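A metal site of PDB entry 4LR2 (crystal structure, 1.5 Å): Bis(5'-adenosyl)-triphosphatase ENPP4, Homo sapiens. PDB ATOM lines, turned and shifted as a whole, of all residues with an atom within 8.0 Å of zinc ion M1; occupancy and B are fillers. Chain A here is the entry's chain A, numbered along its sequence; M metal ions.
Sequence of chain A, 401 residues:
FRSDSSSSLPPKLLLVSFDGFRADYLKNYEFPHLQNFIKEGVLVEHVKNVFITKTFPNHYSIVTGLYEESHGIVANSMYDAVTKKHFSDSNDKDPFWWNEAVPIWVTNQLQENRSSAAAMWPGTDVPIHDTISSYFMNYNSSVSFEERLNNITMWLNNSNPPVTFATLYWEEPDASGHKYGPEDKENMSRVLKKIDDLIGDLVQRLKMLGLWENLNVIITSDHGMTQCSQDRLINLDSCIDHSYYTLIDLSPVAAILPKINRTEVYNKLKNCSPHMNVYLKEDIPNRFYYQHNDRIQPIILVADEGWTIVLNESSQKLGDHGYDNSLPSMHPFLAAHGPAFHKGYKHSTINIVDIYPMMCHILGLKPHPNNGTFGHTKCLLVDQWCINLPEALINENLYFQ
The backbone carbonyl oxygen of Thr 55 lies within hydrogen-bond range of a ring nitrogen (ND1) of His 59, 2.9 Å away. A ring nitrogen (NE2) of His 223 lies close to a ring nitrogen (ND1) of His 321 (3.4 Å). The backbone carbonyl oxygen (O) of His 223 is in hydrogen-bond range of the backbone NH (N) of Phe 21. OD1 of Asp 222 lies within hydrogen-bond range of N of Gly 20 (3.0 Å). The side-chain carboxylate (OD1) of Asp 222 lies within hydrogen-bond range of the side-chain hydroxyl (OG) of Ser 221 (3.2 Å). OD1 of Asn 58 lies close to O of Asp 222 (3.5 Å). OH of Tyr 169 sits at hydrogen-bond distance from OD2 of Asp 19, at 2.7 Å. N of Asp 19 is in hydrogen-bond range of O of Trp 170, 3.0 Å away.
Zinc ion M1 is bound by OG1 of Thr 55 (1.9 Å), NE2 of His 223 (2.0 Å), OD2 of Asp 222 (2.0 Å) and OD1 of Asp 19 (2.0 Å). Slightly farther from zinc ion M1 lies the side-chain carboxylate (OD2) of Asp 19 (2.8 Å).
Four residues have an atom within 4 Å of zinc ion M1: Asp 19, Thr 55, Asp 222 and His 223. Along chain A the residues within 4 Å of zinc ion M1 span positions 19 to 223. The nearest printed residue that does not touch zinc ion M1 is Asp 174 (4.2 Å).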
ATOM      1  N   SER A  17       3.532  26.507  -9.910  1.00  0.00           N
ATOM      2  CA  SER A  17       4.250  26.704  -8.648  1.00  0.00           C
ATOM      3  C   SER A  17       4.922  28.058  -8.673  1.00  0.00           C
ATOM      4  O   SER A  17       5.682  28.361  -9.616  1.00  0.00           O
ATOM      5  CB  SER A  17       5.312  25.628  -8.455  1.00  0.00           C
ATOM      6  OG  SER A  17       6.071  25.891  -7.282  1.00  0.00           O
ATOM      7  N   PHE A  18       4.624  28.886  -7.678  1.00  0.00           N
ATOM      8  CA  PHE A  18       5.420  30.043  -7.369  1.00  0.00           C
ATOM      9  C   PHE A  18       6.346  29.684  -6.212  1.00  0.00           C
ATOM     10  O   PHE A  18       5.902  29.529  -5.063  1.00  0.00           O
ATOM     11  CB  PHE A  18       4.556  31.274  -7.011  1.00  0.00           C
ATOM     12  CG  PHE A  18       3.691  31.726  -8.145  1.00  0.00           C
ATOM     13  CD1 PHE A  18       4.174  32.622  -9.093  1.00  0.00           C
ATOM     14  CD2 PHE A  18       2.376  31.250  -8.286  1.00  0.00           C
ATOM     15  CE1 PHE A  18       3.378  33.038 -10.148  1.00  0.00           C
ATOM     16  CE2 PHE A  18       1.583  31.669  -9.351  1.00  0.00           C
ATOM     17  CZ  PHE A  18       2.081  32.560 -10.273  1.00  0.00           C
ATOM     18  N   ASP A  19       7.620  29.485  -6.528  1.00  0.00           N
ATOM     19  CA  ASP A  19       8.613  29.051  -5.554  1.00  0.00           C
ATOM     20  C   ASP A  19       8.631  29.856  -4.257  1.00  0.00           C
ATOM     21  O   ASP A  19       8.654  31.106  -4.281  1.00  0.00           O
ATOM     22  CB  ASP A  19      10.006  29.064  -6.186  1.00  0.00           C
ATOM     23  CG  ASP A  19      10.955  28.125  -5.472  1.00  0.00           C
ATOM     24  OD1 ASP A  19      11.073  28.199  -4.209  1.00  0.00           O
ATOM     25  OD2 ASP A  19      11.594  27.311  -6.158  1.00  0.00           O
ATOM     26  N   GLY A  20       8.533  29.162  -3.131  1.00  0.00           N
ATOM     27  CA  GLY A  20       8.802  29.789  -1.844  1.00  0.00           C
ATOM     28  C   GLY A  20       7.642  30.608  -1.292  1.00  0.00           C
ATOM     29  O   GLY A  20       7.843  31.602  -0.579  1.00  0.00           O
ATOM     30  N   PHE A  21       6.426  30.184  -1.625  1.00  0.00           N
ATOM     31  CA  PHE A  21       5.208  30.911  -1.236  1.00  0.00           C
ATOM     32  C   PHE A  21       4.711  30.348   0.112  1.00  0.00           C
ATOM     33  O   PHE A  21       3.976  29.349   0.169  1.00  0.00           O
ATOM     34  CB  PHE A  21       4.151  30.816  -2.341  1.00  0.00           C
ATOM     35  CG  PHE A  21       3.084  31.878  -2.246  1.00  0.00           C
ATOM     36  CD1 PHE A  21       2.643  32.511  -3.389  1.00  0.00           C
ATOM     37  CD2 PHE A  21       2.461  32.159  -1.048  1.00  0.00           C
ATOM     38  CE1 PHE A  21       1.623  33.498  -3.332  1.00  0.00           C
ATOM     39  CE2 PHE A  21       1.462  33.134  -0.966  1.00  0.00           C
ATOM     40  CZ  PHE A  21       1.029  33.785  -2.123  1.00  0.00           C
ATOM     41  N   THR A  53      13.027  20.727   3.430  1.00  0.00           N
ATOM     42  CA  THR A  53      12.066  21.607   2.782  1.00  0.00           C
ATOM     43  C   THR A  53      12.741  22.508   1.736  1.00  0.00           C
ATOM     44  O   THR A  53      12.740  23.757   1.845  1.00  0.00           O
ATOM     45  CB  THR A  53      11.204  22.402   3.804  1.00  0.00           C
ATOM     46  OG1 THR A  53      12.065  23.058   4.747  1.00  0.00           O
ATOM     47  CG2 THR A  53      10.278  21.479   4.569  1.00  0.00           C
ATOM     48  N   LYS A  54      13.348  21.863   0.737  1.00  0.00           N
ATOM     49  CA  LYS A  54      14.075  22.552  -0.328  1.00  0.00           C
ATOM     50  C   LYS A  54      13.311  22.391  -1.638  1.00  0.00           C
ATOM     51  O   LYS A  54      12.391  21.575  -1.743  1.00  0.00           O
ATOM     52  CB  LYS A  54      15.485  21.987  -0.449  1.00  0.00           C
ATOM     53  CG  LYS A  54      16.390  22.299   0.752  1.00  0.00           C
ATOM     54  CD  LYS A  54      16.749  23.762   0.840  1.00  0.00           C
ATOM     55  CE  LYS A  54      17.930  23.895   1.799  1.00  0.00           C
ATOM     56  NZ  LYS A  54      18.277  25.322   2.113  1.00  0.00           N
ATOM     57  N   THR A  55      13.766  23.113  -2.663  1.00  0.00           N
ATOM     58  CA  THR A  55      13.030  23.244  -3.929  1.00  0.00           C
ATOM     59  C   THR A  55      12.915  21.998  -4.790  1.00  0.00           C
ATOM     60  O   THR A  55      11.799  21.574  -5.124  1.00  0.00           O
ATOM     61  CB  THR A  55      13.607  24.419  -4.749  1.00  0.00           C
ATOM     62  OG1 THR A  55      13.409  25.640  -4.006  1.00  0.00           O
ATOM     63  CG2 THR A  55      12.950  24.513  -6.139  1.00  0.00           C
ATOM     64  N   PHE A  56      14.039  21.412  -5.172  1.00  0.00           N
ATOM     65  CA  PHE A  56      13.983  20.249  -6.046  1.00  0.00           C
ATOM     66  C   PHE A  56      13.283  19.080  -5.340  1.00  0.00           C
ATOM     67  O   PHE A  56      12.433  18.427  -5.943  1.00  0.00           O
ATOM     68  CB  PHE A  56      15.373  19.906  -6.623  1.00  0.00           C
ATOM     69  CG  PHE A  56      15.718  20.697  -7.861  1.00  0.00           C
ATOM     70  CD1 PHE A  56      15.784  22.084  -7.823  1.00  0.00           C
ATOM     71  CD2 PHE A  56      15.925  20.053  -9.064  1.00  0.00           C
ATOM     72  CE1 PHE A  56      16.100  22.815  -8.956  1.00  0.00           C
ATOM     73  CE2 PHE A  56      16.249  20.777 -10.207  1.00  0.00           C
ATOM     74  CZ  PHE A  56      16.316  22.175 -10.155  1.00  0.00           C
ATOM     75  N   PRO A  57      13.602  18.818  -4.060  1.00  0.00           N
ATOM     76  CA  PRO A  57      12.944  17.667  -3.412  1.00  0.00           C
ATOM     77  C   PRO A  57      11.431  17.836  -3.312  1.00  0.00           C
ATOM     78  O   PRO A  57      10.647  16.895  -3.613  1.00  0.00           O
ATOM     79  CB  PRO A  57      13.567  17.679  -1.993  1.00  0.00           C
ATOM     80  CG  PRO A  57      14.943  18.220  -2.216  1.00  0.00           C
ATOM     81  CD  PRO A  57      14.768  19.294  -3.263  1.00  0.00           C
ATOM     82  N   ASN A  58      10.976  19.029  -2.963  1.00  0.00           N
ATOM     83  CA  ASN A  58       9.523  19.207  -2.820  1.00  0.00           C
ATOM     84  C   ASN A  58       8.762  19.268  -4.134  1.00  0.00           C
ATOM     85  O   ASN A  58       7.636  18.747  -4.204  1.00  0.00           O
ATOM     86  CB  ASN A  58       9.186  20.382  -1.939  1.00  0.00           C
ATOM     87  CG  ASN A  58       9.165  20.008  -0.462  1.00  0.00           C
ATOM     88  OD1 ASN A  58       8.115  19.601   0.065  1.00  0.00           O
ATOM     89  ND2 ASN A  58      10.330  20.109   0.201  1.00  0.00           N
ATOM     90  N   HIS A  59       9.331  19.896  -5.159  1.00  0.00           N
ATOM     91  CA  HIS A  59       8.670  19.841  -6.472  1.00  0.00           C
ATOM     92  C   HIS A  59       8.509  18.375  -6.952  1.00  0.00           C
ATOM     93  O   HIS A  59       7.483  18.001  -7.536  1.00  0.00           O
ATOM     94  CB  HIS A  59       9.363  20.709  -7.543  1.00  0.00           C
ATOM     95  CG  HIS A  59       9.073  22.181  -7.424  1.00  0.00           C
ATOM     96  ND1 HIS A  59       9.798  23.022  -6.594  1.00  0.00           N
ATOM     97  CD2 HIS A  59       8.122  22.957  -7.998  1.00  0.00           C
ATOM     98  CE1 HIS A  59       9.325  24.253  -6.696  1.00  0.00           C
ATOM     99  NE2 HIS A  59       8.307  24.241  -7.538  1.00  0.00           N
ATOM    100  N   ASN A  76      18.961  19.927  -2.878  1.00  0.00           N
ATOM    101  CA  ASN A  76      19.337  20.652  -4.080  1.00  0.00           C
ATOM    102  C   ASN A  76      20.764  20.354  -4.524  1.00  0.00           C
ATOM    103  O   ASN A  76      21.101  20.610  -5.670  1.00  0.00           O
ATOM    104  CB  ASN A  76      19.124  22.166  -3.913  1.00  0.00           C
ATOM    105  CG  ASN A  76      17.809  22.648  -4.522  1.00  0.00           C
ATOM    106  OD1 ASN A  76      16.754  22.009  -4.341  1.00  0.00           O
ATOM    107  ND2 ASN A  76      17.872  23.747  -5.290  1.00  0.00           N
ATOM    108  N   PRO A 122      11.098  22.073 -12.398  1.00  0.00           N
ATOM    109  CA  PRO A 122      12.288  21.244 -12.162  1.00  0.00           C
ATOM    110  C   PRO A 122      12.154  19.822 -12.698  1.00  0.00           C
ATOM    111  O   PRO A 122      11.183  19.105 -12.369  1.00  0.00           O
ATOM    112  CB  PRO A 122      12.401  21.238 -10.640  1.00  0.00           C
ATOM    113  CG  PRO A 122      11.850  22.546 -10.248  1.00  0.00           C
ATOM    114  CD  PRO A 122      10.681  22.766 -11.174  1.00  0.00           C
ATOM    115  N   TYR A 169       6.252  27.168 -13.823  1.00  0.00           N
ATOM    116  CA  TYR A 169       7.082  27.462 -12.651  1.00  0.00           C
ATOM    117  C   TYR A 169       7.620  28.889 -12.688  1.00  0.00           C
ATOM    118  O   TYR A 169       7.952  29.426 -13.760  1.00  0.00           O
ATOM    119  CB  TYR A 169       8.251  26.483 -12.592  1.00  0.00           C
ATOM    120  CG  TYR A 169       9.330  26.820 -11.578  1.00  0.00           C
ATOM    121  CD1 TYR A 169       9.239  26.383 -10.271  1.00  0.00           C
ATOM    122  CD2 TYR A 169      10.442  27.565 -11.951  1.00  0.00           C
ATOM    123  CE1 TYR A 169      10.217  26.678  -9.334  1.00  0.00           C
ATOM    124  CE2 TYR A 169      11.431  27.880 -11.037  1.00  0.00           C
ATOM    125  CZ  TYR A 169      11.324  27.445  -9.724  1.00  0.00           C
ATOM    126  OH  TYR A 169      12.310  27.755  -8.769  1.00  0.00           O
ATOM    127  N   TRP A 170       7.714  29.504 -11.515  1.00  0.00           N
ATOM    128  CA  TRP A 170       8.254  30.862 -11.397  1.00  0.00           C
ATOM    129  C   TRP A 170       9.144  30.907 -10.165  1.00  0.00           C
ATOM    130  O   TRP A 170       8.857  30.205  -9.178  1.00  0.00           O
ATOM    131  CB  TRP A 170       7.134  31.893 -11.307  1.00  0.00           C
ATOM    132  CG  TRP A 170       7.592  33.310 -11.373  1.00  0.00           C
ATOM    133  CD1 TRP A 170       7.406  34.267 -10.426  1.00  0.00           C
ATOM    134  CD2 TRP A 170       8.294  33.951 -12.460  1.00  0.00           C
ATOM    135  NE1 TRP A 170       7.966  35.457 -10.835  1.00  0.00           N
ATOM    136  CE2 TRP A 170       8.501  35.290 -12.086  1.00  0.00           C
ATOM    137  CE3 TRP A 170       8.776  33.507 -13.694  1.00  0.00           C
ATOM    138  CZ2 TRP A 170       9.168  36.192 -12.907  1.00  0.00           C
ATOM    139  CZ3 TRP A 170       9.427  34.411 -14.509  1.00  0.00           C
ATOM    140  CH2 TRP A 170       9.617  35.738 -14.111  1.00  0.00           C
ATOM    141  N   GLU A 171      10.205  31.713 -10.213  1.00  0.00           N
ATOM    142  CA  GLU A 171      11.250  31.703  -9.194  1.00  0.00           C
ATOM    143  C   GLU A 171      10.949  32.534  -7.961  1.00  0.00           C
ATOM    144  O   GLU A 171      11.660  32.420  -6.948  1.00  0.00           O
ATOM    145  CB  GLU A 171      12.579  32.232  -9.773  1.00  0.00           C
ATOM    146  CG  GLU A 171      13.262  31.308 -10.789  1.00  0.00           C
ATOM    147  CD  GLU A 171      12.639  31.374 -12.166  1.00  0.00           C
ATOM    148  OE1 GLU A 171      12.926  30.491 -12.995  1.00  0.00           O
ATOM    149  OE2 GLU A 171      11.855  32.317 -12.425  1.00  0.00           O
ATOM    150  N   ASP A 174      10.425  33.070  -3.786  1.00  0.00           N
ATOM    151  CA  ASP A 174      11.585  32.491  -3.102  1.00  0.00           C
ATOM    152  C   ASP A 174      12.844  33.370  -3.185  1.00  0.00           C
ATOM    153  O   ASP A 174      13.460  33.677  -2.177  1.00  0.00           O
ATOM    154  CB  ASP A 174      11.882  31.118  -3.691  1.00  0.00           C
ATOM    155  CG  ASP A 174      12.985  30.382  -2.937  1.00  0.00           C
ATOM    156  OD1 ASP A 174      12.788  30.045  -1.758  1.00  0.00           O
ATOM    157  OD2 ASP A 174      14.044  30.112  -3.526  1.00  0.00           O
ATOM    158  N   ALA A 175      13.207  33.774  -4.402  1.00  0.00           N
ATOM    159  CA  ALA A 175      14.421  34.555  -4.613  1.00  0.00           C
ATOM    160  C   ALA A 175      14.471  35.807  -3.727  1.00  0.00           C
ATOM    161  O   ALA A 175      15.494  36.068  -3.055  1.00  0.00           O
ATOM    162  CB  ALA A 175      14.565  34.956  -6.096  1.00  0.00           C
ATOM    163  N   HIS A 178      14.632  35.189   0.140  1.00  0.00           N
ATOM    164  CA  HIS A 178      16.010  34.966   0.601  1.00  0.00           C
ATOM    165  C   HIS A 178      16.705  36.294   0.793  1.00  0.00           C
ATOM    166  O   HIS A 178      17.396  36.518   1.792  1.00  0.00           O
ATOM    167  CB  HIS A 178      16.809  34.145  -0.416  1.00  0.00           C
ATOM    168  CG  HIS A 178      16.516  32.676  -0.376  1.00  0.00           C
ATOM    169  ND1 HIS A 178      16.724  31.917   0.756  1.00  0.00           N
ATOM    170  CD2 HIS A 178      16.029  31.833  -1.314  1.00  0.00           C
ATOM    171  CE1 HIS A 178      16.383  30.663   0.513  1.00  0.00           C
ATOM    172  NE2 HIS A 178      15.952  30.590  -0.741  1.00  0.00           N
ATOM    173  N   SER A 221       2.901  25.726  -4.173  1.00  0.00           N
ATOM    174  CA  SER A 221       4.311  26.036  -4.014  1.00  0.00           C
ATOM    175  C   SER A 221       5.016  24.884  -3.316  1.00  0.00           C
ATOM    176  O   SER A 221       4.386  23.857  -3.005  1.00  0.00           O
ATOM    177  CB  SER A 221       4.525  27.348  -3.254  1.00  0.00           C
ATOM    178  OG  SER A 221       5.902  27.726  -3.185  1.00  0.00           O
ATOM    179  N   ASP A 222       6.306  25.046  -3.095  1.00  0.00           N
ATOM    180  CA  ASP A 222       7.113  23.958  -2.586  1.00  0.00           C
ATOM    181  C   ASP A 222       7.438  24.067  -1.095  1.00  0.00           C
ATOM    182  O   ASP A 222       7.655  23.026  -0.438  1.00  0.00           O
ATOM    183  CB  ASP A 222       8.380  23.796  -3.425  1.00  0.00           C
ATOM    184  CG  ASP A 222       9.232  25.075  -3.510  1.00  0.00           C
ATOM    185  OD1 ASP A 222       8.733  26.202  -3.225  1.00  0.00           O
ATOM    186  OD2 ASP A 222      10.411  24.922  -3.941  1.00  0.00           O
ATOM    187  N   HIS A 223       7.439  25.283  -0.560  1.00  0.00           N
ATOM    188  CA  HIS A 223       7.850  25.521   0.830  1.00  0.00           C
ATOM    189  C   HIS A 223       7.722  26.996   1.100  1.00  0.00           C
ATOM    190  O   HIS A 223       7.438  27.784   0.201  1.00  0.00           O
ATOM    191  CB  HIS A 223       9.334  25.169   1.062  1.00  0.00           C
ATOM    192  CG  HIS A 223      10.257  25.850   0.090  1.00  0.00           C
ATOM    193  ND1 HIS A 223      10.554  27.197   0.159  1.00  0.00           N
ATOM    194  CD2 HIS A 223      10.922  25.375  -0.996  1.00  0.00           C
ATOM    195  CE1 HIS A 223      11.322  27.535  -0.869  1.00  0.00           C
ATOM    196  NE2 HIS A 223      11.585  26.430  -1.571  1.00  0.00           N
ATOM    197  N   GLY A 224       7.937  27.361   2.364  1.00  0.00           N
ATOM    198  CA  GLY A 224       7.895  28.733   2.808  1.00  0.00           C
ATOM    199  C   GLY A 224       9.265  29.318   3.017  1.00  0.00           C
ATOM    200  O   GLY A 224      10.190  29.043   2.221  1.00  0.00           O
ATOM    201  N   MET A 225       9.398  30.116   4.079  1.00  0.00           N
ATOM    202  CA  MET A 225      10.613  30.921   4.308  1.00  0.00           C
ATOM    203  C   MET A 225      10.601  31.358   5.757  1.00  0.00           C
ATOM    204  O   MET A 225       9.524  31.610   6.302  1.00  0.00           O
ATOM    205  CB  MET A 225      10.627  32.143   3.395  1.00  0.00           C
ATOM    206  CG  MET A 225      11.970  32.866   3.264  1.00  0.00           C
ATOM    207  SD  MET A 225      13.305  32.014   2.380  1.00  0.00           S
ATOM    208  CE  MET A 225      12.613  31.981   0.716  1.00  0.00           C
ATOM    209  N   HIS A 321      14.978  28.409   3.932  1.00  0.00           N
ATOM    210  CA  HIS A 321      14.077  27.289   4.141  1.00  0.00           C
ATOM    211  C   HIS A 321      14.897  26.007   4.093  1.00  0.00           C
ATOM    212  O   HIS A 321      16.108  26.016   3.770  1.00  0.00           O
ATOM    213  CB  HIS A 321      12.994  27.247   3.054  1.00  0.00           C
ATOM    214  CG  HIS A 321      13.524  27.321   1.661  1.00  0.00           C
ATOM    215  ND1 HIS A 321      13.860  26.204   0.925  1.00  0.00           N
ATOM    216  CD2 HIS A 321      13.880  28.384   0.891  1.00  0.00           C
ATOM    217  CE1 HIS A 321      14.351  26.564  -0.251  1.00  0.00           C
ATOM    218  NE2 HIS A 321      14.378  27.887  -0.287  1.00  0.00           N
HETATM  219 ZN    ZN M   1      11.717  26.398  -3.566  1.00  0.00          ZN
HETATM  220 ZN    ZN M   2      15.147  29.013  -1.850  1.00  0.00          ZN
